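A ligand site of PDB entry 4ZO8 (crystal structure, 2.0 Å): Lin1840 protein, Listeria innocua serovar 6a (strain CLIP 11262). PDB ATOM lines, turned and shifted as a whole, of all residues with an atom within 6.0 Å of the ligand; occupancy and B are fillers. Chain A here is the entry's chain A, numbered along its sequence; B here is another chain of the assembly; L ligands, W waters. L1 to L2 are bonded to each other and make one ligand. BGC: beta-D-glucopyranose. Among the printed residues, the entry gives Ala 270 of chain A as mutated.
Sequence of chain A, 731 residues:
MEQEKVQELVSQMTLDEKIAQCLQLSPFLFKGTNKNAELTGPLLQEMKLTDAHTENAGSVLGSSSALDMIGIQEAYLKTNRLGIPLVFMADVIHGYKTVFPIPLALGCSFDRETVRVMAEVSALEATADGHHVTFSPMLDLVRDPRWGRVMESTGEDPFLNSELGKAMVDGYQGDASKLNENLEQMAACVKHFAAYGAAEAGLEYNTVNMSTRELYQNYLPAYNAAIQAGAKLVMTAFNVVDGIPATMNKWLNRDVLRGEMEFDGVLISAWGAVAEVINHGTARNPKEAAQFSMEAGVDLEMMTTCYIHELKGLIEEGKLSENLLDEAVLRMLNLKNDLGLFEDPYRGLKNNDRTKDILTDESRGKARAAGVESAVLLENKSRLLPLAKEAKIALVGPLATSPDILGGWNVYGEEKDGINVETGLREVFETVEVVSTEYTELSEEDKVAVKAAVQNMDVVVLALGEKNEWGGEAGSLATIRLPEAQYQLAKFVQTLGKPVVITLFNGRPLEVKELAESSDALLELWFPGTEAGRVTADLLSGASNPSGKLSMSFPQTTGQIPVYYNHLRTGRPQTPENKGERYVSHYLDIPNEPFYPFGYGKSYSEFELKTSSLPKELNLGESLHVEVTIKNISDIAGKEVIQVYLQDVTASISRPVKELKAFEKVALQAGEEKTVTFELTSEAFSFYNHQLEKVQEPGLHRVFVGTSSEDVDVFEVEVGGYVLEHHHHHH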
ATOM      1  N   LEU A  61      -7.334  26.434  15.510  1.00  0.00           N
ATOM      2  CA  LEU A  61      -6.262  25.509  15.869  1.00  0.00           C
ATOM      3  C   LEU A  61      -6.290  25.229  17.359  1.00  0.00           C
ATOM      4  O   LEU A  61      -6.036  26.106  18.155  1.00  0.00           O
ATOM      5  CB  LEU A  61      -4.909  26.212  15.580  1.00  0.00           C
ATOM      6  CG  LEU A  61      -3.597  25.531  16.019  1.00  0.00           C
ATOM      7  CD1 LEU A  61      -3.030  24.552  15.050  1.00  0.00           C
ATOM      8  CD2 LEU A  61      -2.537  26.574  16.255  1.00  0.00           C
ATOM      9  N   ASP A  91      -3.995  18.454  16.981  1.00  0.00           N
ATOM     10  CA  ASP A  91      -2.936  17.475  17.065  1.00  0.00           C
ATOM     11  C   ASP A  91      -3.416  16.243  17.855  1.00  0.00           C
ATOM     12  O   ASP A  91      -3.355  16.202  19.094  1.00  0.00           O
ATOM     13  CB  ASP A  91      -1.730  18.088  17.777  1.00  0.00           C
ATOM     14  CG  ASP A  91      -0.981  19.076  16.913  1.00  0.00           C
ATOM     15  OD1 ASP A  91      -0.585  18.697  15.807  1.00  0.00           O
ATOM     16  OD2 ASP A  91      -0.746  20.211  17.321  1.00  0.00           O
ATOM     17  N   ILE A  93      -2.179  12.752  17.704  1.00  0.00           N
ATOM     18  CA  ILE A  93      -0.974  12.140  17.180  1.00  0.00           C
ATOM     19  C   ILE A  93      -0.924  10.647  17.497  1.00  0.00           C
ATOM     20  O   ILE A  93      -0.599   9.827  16.657  1.00  0.00           O
ATOM     21  CB  ILE A  93       0.278  12.852  17.756  1.00  0.00           C
ATOM     22  CG1 ILE A  93       0.162  14.359  17.562  1.00  0.00           C
ATOM     23  CG2 ILE A  93       1.558  12.288  17.111  1.00  0.00           C
ATOM     24  CD1 ILE A  93      -0.086  14.745  16.084  1.00  0.00           C
ATOM     25  N   PHE A 135      -3.719  16.651  12.840  1.00  0.00           N
ATOM     26  CA  PHE A 135      -2.406  16.834  12.206  1.00  0.00           C
ATOM     27  C   PHE A 135      -1.558  15.575  12.365  1.00  0.00           C
ATOM     28  O   PHE A 135      -0.496  15.559  13.000  1.00  0.00           O
ATOM     29  CB  PHE A 135      -1.664  18.051  12.772  1.00  0.00           C
ATOM     30  CG  PHE A 135      -2.392  19.349  12.629  1.00  0.00           C
ATOM     31  CD1 PHE A 135      -2.808  19.795  11.371  1.00  0.00           C
ATOM     32  CD2 PHE A 135      -2.715  20.116  13.753  1.00  0.00           C
ATOM     33  CE1 PHE A 135      -3.489  20.990  11.235  1.00  0.00           C
ATOM     34  CE2 PHE A 135      -3.332  21.324  13.614  1.00  0.00           C
ATOM     35  CZ  PHE A 135      -3.722  21.770  12.330  1.00  0.00           C
ATOM     36  N   ARG A 149      11.954  14.497  17.507  1.00  0.00           N
ATOM     37  CA  ARG A 149      10.714  14.148  16.800  1.00  0.00           C
ATOM     38  C   ARG A 149      10.679  12.755  16.197  1.00  0.00           C
ATOM     39  O   ARG A 149       9.684  12.385  15.614  1.00  0.00           O
ATOM     40  CB  ARG A 149      10.336  15.202  15.736  1.00  0.00           C
ATOM     41  CG  ARG A 149      10.374  16.595  16.319  1.00  0.00           C
ATOM     42  CD  ARG A 149       9.678  17.532  15.395  1.00  0.00           C
ATOM     43  NE  ARG A 149       8.243  17.452  15.569  1.00  0.00           N
ATOM     44  CZ  ARG A 149       7.346  18.357  15.173  1.00  0.00           C
ATOM     45  NH1 ARG A 149       7.718  19.492  14.652  1.00  0.00           N
ATOM     46  NH2 ARG A 149       6.043  18.128  15.395  1.00  0.00           N
ATOM     47  N   GLU A 152       7.559  10.628  16.764  1.00  0.00           N
ATOM     48  CA  GLU A 152       6.321  10.824  15.943  1.00  0.00           C
ATOM     49  C   GLU A 152       6.351  10.094  14.609  1.00  0.00           C
ATOM     50  O   GLU A 152       5.343   9.997  13.901  1.00  0.00           O
ATOM     51  CB  GLU A 152       6.110  12.287  15.615  1.00  0.00           C
ATOM     52  CG  GLU A 152       5.962  13.268  16.761  1.00  0.00           C
ATOM     53  CD  GLU A 152       6.289  14.681  16.283  1.00  0.00           C
ATOM     54  OE1 GLU A 152       5.592  15.224  15.381  1.00  0.00           O
ATOM     55  OE2 GLU A 152       7.259  15.256  16.832  1.00  0.00           O
ATOM     56  N   LYS A 191       2.000  15.176   7.481  1.00  0.00           N
ATOM     57  CA  LYS A 191       3.071  16.187   7.769  1.00  0.00           C
ATOM     58  C   LYS A 191       4.439  15.478   7.853  1.00  0.00           C
ATOM     59  O   LYS A 191       4.472  14.221   7.934  1.00  0.00           O
ATOM     60  CB  LYS A 191       2.678  17.028   9.014  1.00  0.00           C
ATOM     61  CG  LYS A 191       2.818  16.280  10.328  1.00  0.00           C
ATOM     62  CD  LYS A 191       2.035  16.909  11.482  1.00  0.00           C
ATOM     63  CE  LYS A 191       2.530  16.417  12.821  1.00  0.00           C
ATOM     64  NZ  LYS A 191       1.702  16.934  13.960  1.00  0.00           N
ATOM     65  N   HIS A 192       5.549  16.179   7.754  1.00  0.00           N
ATOM     66  CA  HIS A 192       5.700  17.603   7.454  1.00  0.00           C
ATOM     67  C   HIS A 192       6.337  17.624   6.086  1.00  0.00           C
ATOM     68  O   HIS A 192       7.446  17.117   5.923  1.00  0.00           O
ATOM     69  CB  HIS A 192       6.651  18.261   8.455  1.00  0.00           C
ATOM     70  CG  HIS A 192       6.209  18.194   9.879  1.00  0.00           C
ATOM     71  ND1 HIS A 192       6.411  17.077  10.668  1.00  0.00           N
ATOM     72  CD2 HIS A 192       5.623  19.115  10.685  1.00  0.00           C
ATOM     73  CE1 HIS A 192       5.955  17.301  11.878  1.00  0.00           C
ATOM     74  NE2 HIS A 192       5.468  18.522  11.918  1.00  0.00           N
ATOM     75  N   TYR A 196      11.812  16.639   6.755  1.00  0.00           N
ATOM     76  CA  TYR A 196      12.088  17.331   8.019  1.00  0.00           C
ATOM     77  C   TYR A 196      13.000  16.539   8.981  1.00  0.00           C
ATOM     78  O   TYR A 196      13.871  17.111   9.668  1.00  0.00           O
ATOM     79  CB  TYR A 196      10.719  17.658   8.663  1.00  0.00           C
ATOM     80  CG  TYR A 196      10.679  18.384   9.965  1.00  0.00           C
ATOM     81  CD1 TYR A 196      11.639  19.334  10.340  1.00  0.00           C
ATOM     82  CD2 TYR A 196       9.640  18.195  10.817  1.00  0.00           C
ATOM     83  CE1 TYR A 196      11.535  20.028  11.573  1.00  0.00           C
ATOM     84  CE2 TYR A 196       9.533  18.871  12.010  1.00  0.00           C
ATOM     85  CZ  TYR A 196      10.483  19.759  12.384  1.00  0.00           C
ATOM     86  OH  TYR A 196      10.337  20.328  13.622  1.00  0.00           O
ATOM     87  N   TYR A 205      14.844  22.056  13.766  1.00  0.00           N
ATOM     88  CA  TYR A 205      14.629  23.020  12.654  1.00  0.00           C
ATOM     89  C   TYR A 205      15.844  23.225  11.734  1.00  0.00           C
ATOM     90  O   TYR A 205      15.783  24.044  10.784  1.00  0.00           O
ATOM     91  CB  TYR A 205      14.126  24.399  13.165  1.00  0.00           C
ATOM     92  CG  TYR A 205      13.113  24.314  14.303  1.00  0.00           C
ATOM     93  CD1 TYR A 205      11.830  23.832  14.085  1.00  0.00           C
ATOM     94  CD2 TYR A 205      13.456  24.732  15.627  1.00  0.00           C
ATOM     95  CE1 TYR A 205      10.914  23.750  15.104  1.00  0.00           C
ATOM     96  CE2 TYR A 205      12.518  24.717  16.643  1.00  0.00           C
ATOM     97  CZ  TYR A 205      11.260  24.191  16.398  1.00  0.00           C
ATOM     98  OH  TYR A 205      10.236  24.145  17.352  1.00  0.00           O
ATOM     99  N   MET A 235       0.597  19.326   5.419  1.00  0.00           N
ATOM    100  CA  MET A 235       1.235  20.450   6.153  1.00  0.00           C
ATOM    101  C   MET A 235       2.720  20.637   5.683  1.00  0.00           C
ATOM    102  O   MET A 235       3.454  19.668   5.533  1.00  0.00           O
ATOM    103  CB  MET A 235       1.110  20.238   7.701  1.00  0.00           C
ATOM    104  CG  MET A 235       1.743  21.301   8.577  1.00  0.00           C
ATOM    105  SD  MET A 235       1.985  20.912  10.335  1.00  0.00           S
ATOM    106  CE  MET A 235       0.240  20.911  10.841  1.00  0.00           C
ATOM    107  N   PHE A 238       9.200  22.899   8.436  1.00  0.00           N
ATOM    108  CA  PHE A 238      10.067  23.971   8.868  1.00  0.00           C
ATOM    109  C   PHE A 238      11.417  24.162   8.158  1.00  0.00           C
ATOM    110  O   PHE A 238      11.907  25.333   8.075  1.00  0.00           O
ATOM    111  CB  PHE A 238      10.338  23.831  10.357  1.00  0.00           C
ATOM    112  CG  PHE A 238       9.119  24.069  11.233  1.00  0.00           C
ATOM    113  CD1 PHE A 238       8.526  25.308  11.290  1.00  0.00           C
ATOM    114  CD2 PHE A 238       8.592  23.052  12.016  1.00  0.00           C
ATOM    115  CE1 PHE A 238       7.459  25.562  12.106  1.00  0.00           C
ATOM    116  CE2 PHE A 238       7.487  23.280  12.847  1.00  0.00           C
ATOM    117  CZ  PHE A 238       6.911  24.524  12.876  1.00  0.00           C
ATOM    118  N   ALA A 270       3.058  24.764   8.602  1.00  0.00           N
ATOM    119  CA  ALA A 270       3.377  24.405   9.988  1.00  0.00           C
ATOM    120  C   ALA A 270       3.291  25.688  10.817  1.00  0.00           C
ATOM    121  O   ALA A 270       3.249  26.799  10.251  1.00  0.00           O
ATOM    122  CB  ALA A 270       4.727  23.816  10.078  1.00  0.00           C
ATOM    123  N   TRP A 271       3.347  25.567  12.126  1.00  0.00           N
ATOM    124  CA  TRP A 271       3.141  26.730  12.971  1.00  0.00           C
ATOM    125  C   TRP A 271       4.152  27.852  12.696  1.00  0.00           C
ATOM    126  O   TRP A 271       5.348  27.686  12.855  1.00  0.00           O
ATOM    127  CB  TRP A 271       3.205  26.351  14.404  1.00  0.00           C
ATOM    128  CG  TRP A 271       2.973  27.537  15.275  1.00  0.00           C
ATOM    129  CD1 TRP A 271       3.753  28.662  15.382  1.00  0.00           C
ATOM    130  CD2 TRP A 271       1.899  27.711  16.181  1.00  0.00           C
ATOM    131  NE1 TRP A 271       3.217  29.529  16.286  1.00  0.00           N
ATOM    132  CE2 TRP A 271       2.095  28.964  16.816  1.00  0.00           C
ATOM    133  CE3 TRP A 271       0.832  26.925  16.558  1.00  0.00           C
ATOM    134  CZ2 TRP A 271       1.217  29.463  17.756  1.00  0.00           C
ATOM    135  CZ3 TRP A 271      -0.039  27.429  17.540  1.00  0.00           C
ATOM    136  CH2 TRP A 271       0.154  28.677  18.104  1.00  0.00           C
ATOM    137  N   MET A 302      -0.819  29.243   9.509  1.00  0.00           N
ATOM    138  CA  MET A 302      -1.080  28.906  10.909  1.00  0.00           C
ATOM    139  C   MET A 302      -0.459  29.888  11.904  1.00  0.00           C
ATOM    140  O   MET A 302       0.762  29.905  12.156  1.00  0.00           O
ATOM    141  CB  MET A 302      -0.589  27.494  11.203  1.00  0.00           C
ATOM    142  CG  MET A 302      -0.685  27.049  12.655  1.00  0.00           C
ATOM    143  SD  MET A 302      -0.016  25.412  12.953  1.00  0.00           S
ATOM    144  CE  MET A 302      -1.031  24.348  11.967  1.00  0.00           C
ATOM    145  N   TRP A 409       3.840  14.556  22.546  1.00  0.00           N
ATOM    146  CA  TRP A 409       2.741  14.853  21.663  1.00  0.00           C
ATOM    147  C   TRP A 409       1.417  14.223  22.187  1.00  0.00           C
ATOM    148  O   TRP A 409       0.618  13.605  21.469  1.00  0.00           O
ATOM    149  CB  TRP A 409       3.117  14.482  20.232  1.00  0.00           C
ATOM    150  CG  TRP A 409       3.838  15.596  19.555  1.00  0.00           C
ATOM    151  CD1 TRP A 409       5.142  15.578  19.142  1.00  0.00           C
ATOM    152  CD2 TRP A 409       3.337  16.901  19.260  1.00  0.00           C
ATOM    153  NE1 TRP A 409       5.471  16.781  18.605  1.00  0.00           N
ATOM    154  CE2 TRP A 409       4.389  17.627  18.690  1.00  0.00           C
ATOM    155  CE3 TRP A 409       2.087  17.525  19.404  1.00  0.00           C
ATOM    156  CZ2 TRP A 409       4.230  18.928  18.198  1.00  0.00           C
ATOM    157  CZ3 TRP A 409       1.924  18.857  18.983  1.00  0.00           C
ATOM    158  CH2 TRP A 409       2.992  19.543  18.384  1.00  0.00           C
ATOM    159  N   GLU A 473       8.925  17.883  19.884  1.00  0.00           N
ATOM    160  CA  GLU A 473       9.440  19.079  19.199  1.00  0.00           C
ATOM    161  C   GLU A 473      10.392  19.923  20.067  1.00  0.00           C
ATOM    162  O   GLU A 473      10.075  20.306  21.194  1.00  0.00           O
ATOM    163  CB  GLU A 473       8.326  19.986  18.745  1.00  0.00           C
ATOM    164  CG  GLU A 473       8.833  21.118  17.878  1.00  0.00           C
ATOM    165  CD  GLU A 473       7.742  22.052  17.356  1.00  0.00           C
ATOM    166  OE1 GLU A 473       6.515  21.647  17.427  1.00  0.00           O
ATOM    167  OE2 GLU A 473       8.122  23.178  16.906  1.00  0.00           O
ATOM    168  N   ARG B 572      14.026  29.180  12.926  1.00  0.00           N
ATOM    169  CA  ARG B 572      13.903  29.593  14.320  1.00  0.00           C
ATOM    170  C   ARG B 572      15.251  29.728  15.083  1.00  0.00           C
ATOM    171  O   ARG B 572      15.479  29.014  16.045  1.00  0.00           O
ATOM    172  CB  ARG B 572      12.964  28.643  15.048  1.00  0.00           C
ATOM    173  CG  ARG B 572      11.554  28.640  14.488  1.00  0.00           C
ATOM    174  CD  ARG B 572      10.703  27.612  15.198  1.00  0.00           C
ATOM    175  NE  ARG B 572       9.303  27.663  14.770  1.00  0.00           N
ATOM    176  CZ  ARG B 572       8.278  27.151  15.464  1.00  0.00           C
ATOM    177  NH1 ARG B 572       8.451  26.542  16.640  1.00  0.00           N
ATOM    178  NH2 ARG B 572       7.059  27.281  15.000  1.00  0.00           N
ATOM    179  N   TYR B 583      10.873  26.572  21.893  1.00  0.00           N
ATOM    180  CA  TYR B 583      10.695  26.425  20.468  1.00  0.00           C
ATOM    181  C   TYR B 583      11.659  27.250  19.573  1.00  0.00           C
ATOM    182  O   TYR B 583      11.248  28.113  18.778  1.00  0.00           O
ATOM    183  CB  TYR B 583       9.251  26.660  20.145  1.00  0.00           C
ATOM    184  CG  TYR B 583       8.396  25.615  20.814  1.00  0.00           C
ATOM    185  CD1 TYR B 583       8.396  24.298  20.326  1.00  0.00           C
ATOM    186  CD2 TYR B 583       7.604  25.926  21.908  1.00  0.00           C
ATOM    187  CE1 TYR B 583       7.627  23.314  20.925  1.00  0.00           C
ATOM    188  CE2 TYR B 583       6.820  24.947  22.555  1.00  0.00           C
ATOM    189  CZ  TYR B 583       6.829  23.648  22.069  1.00  0.00           C
ATOM    190  OH  TYR B 583       6.060  22.686  22.668  1.00  0.00           O
HETATM  191  C2  BGC L   1       3.753  24.220  17.321  1.00  0.00           C
HETATM  192  C3  BGC L   1       5.242  24.726  17.455  1.00  0.00           C
HETATM  193  C4  BGC L   1       5.130  26.093  18.049  1.00  0.00           C
HETATM  194  C5  BGC L   1       4.326  26.012  19.416  1.00  0.00           C
HETATM  195  C6  BGC L   1       4.279  27.356  20.018  1.00  0.00           C
HETATM  196  C1  BGC L   1       3.092  24.257  18.676  1.00  0.00           C
HETATM  197  O1  BGC L   1       1.701  24.045  18.433  1.00  0.00           O
HETATM  198  O2  BGC L   1       3.607  22.851  16.875  1.00  0.00           O
HETATM  199  O3  BGC L   1       6.006  24.777  16.184  1.00  0.00           O
HETATM  200  O4  BGC L   1       6.469  26.588  18.324  1.00  0.00           O
HETATM  201  O5  BGC L   1       3.008  25.522  19.254  1.00  0.00           O
HETATM  202  O6  BGC L   1       3.137  27.333  20.845  1.00  0.00           O
HETATM  203  C2  BGC L   2       4.221  21.260  15.240  1.00  0.00           C
HETATM  204  C3  BGC L   2       3.310  20.481  14.235  1.00  0.00           C
HETATM  205  C4  BGC L   2       1.866  20.603  14.659  1.00  0.00           C
HETATM  206  C5  BGC L   2       1.481  22.000  14.278  1.00  0.00           C
HETATM  207  C6  BGC L   2       0.122  22.350  14.853  1.00  0.00           C
HETATM  208  C1  BGC L   2       3.677  22.666  15.483  1.00  0.00           C
HETATM  209  O2  BGC L   2       5.580  21.296  14.794  1.00  0.00           O
HETATM  210  O3  BGC L   2       3.631  19.150  14.083  1.00  0.00           O
HETATM  211  O4  BGC L   2       1.083  19.762  13.974  1.00  0.00           O
HETATM  212  O5  BGC L   2       2.527  23.008  14.653  1.00  0.00           O
HETATM  213  O6  BGC L   2       0.354  22.371  16.235  1.00  0.00           O
HETATM  214  O   HOH W   1       6.578  29.136  18.336  1.00  0.00           O
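NH1 of Arg 572 of chain B lies within hydrogen-bond range of OH of Tyr 205 (3.1 Å). OH of Tyr 196 sits at hydrogen-bond distance from NH1 of Arg 149 (2.9 Å). The side-chain amino group (NZ) of Lys 191 lies within salt-bridge range of the side-chain carboxylate (OD1) of Asp 91 (3.4 Å). OE2 of Glu 473 is in salt-bridge range of NH1 of Arg 572 of chain B, 3.4 Å away. N of Trp 271 lies close to SD of Met 302. The backbone carbonyl oxygen of Trp 271 is in hydrogen-bond range of the guanidinium group of Arg 572 of chain B (2.8 Å). NZ of Lys 191 is in hydrogen-bond range of O of Phe 135 (2.8 Å). The guanidinium group (NH1) of Arg 149 is in salt-bridge range of the side-chain carboxylate (OE1) of Glu 473.
The side-chain amino group (NZ) of Lys 191 is in hydrogen-bond range of an oxygen (O4) of BGC L2, at 2.9 Å. O3 of BGC L2 sits at hydrogen-bond distance from NE2 of His 192 (2.9 Å). An oxygen (O6) of BGC L2 is in hydrogen-bond range of the side-chain carboxylate of Asp 91, 2.7 Å away. The guanidinium group (NH1) of Arg 149 lies within hydrogen-bond range of an oxygen (O2) of BGC L2, 2.8 Å away. The guanidinium group (NH1) of Arg 572 of chain B lies within hydrogen-bond range of an oxygen (O4) of BGC L1, 2.6 Å away. O3 of BGC L1 lies within hydrogen-bond range of OE2 of Glu 473 (2.7 Å).
Residues that only touch the ligand: Leu 61, Phe 135, Met 235, Phe 238, Trp 271, Met 302, Trp 409 and Tyr 583 of chain B. Hydrophobic or aromatic side chains within 4 Å of the ligand: Leu 61, Phe 135, His 192, Met 235, Phe 238, Trp 271, Met 302, Trp 409 and Tyr 583 of chain B. 14 residues have an atom within 4 Å of the ligand: Leu 61, Asp 91, Phe 135, Arg 149, Lys 191, His 192, Met 235, Phe 238, Trp 271, Met 302, Trp 409, Glu 473, Arg 572 of chain B and Tyr 583 of chain B.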
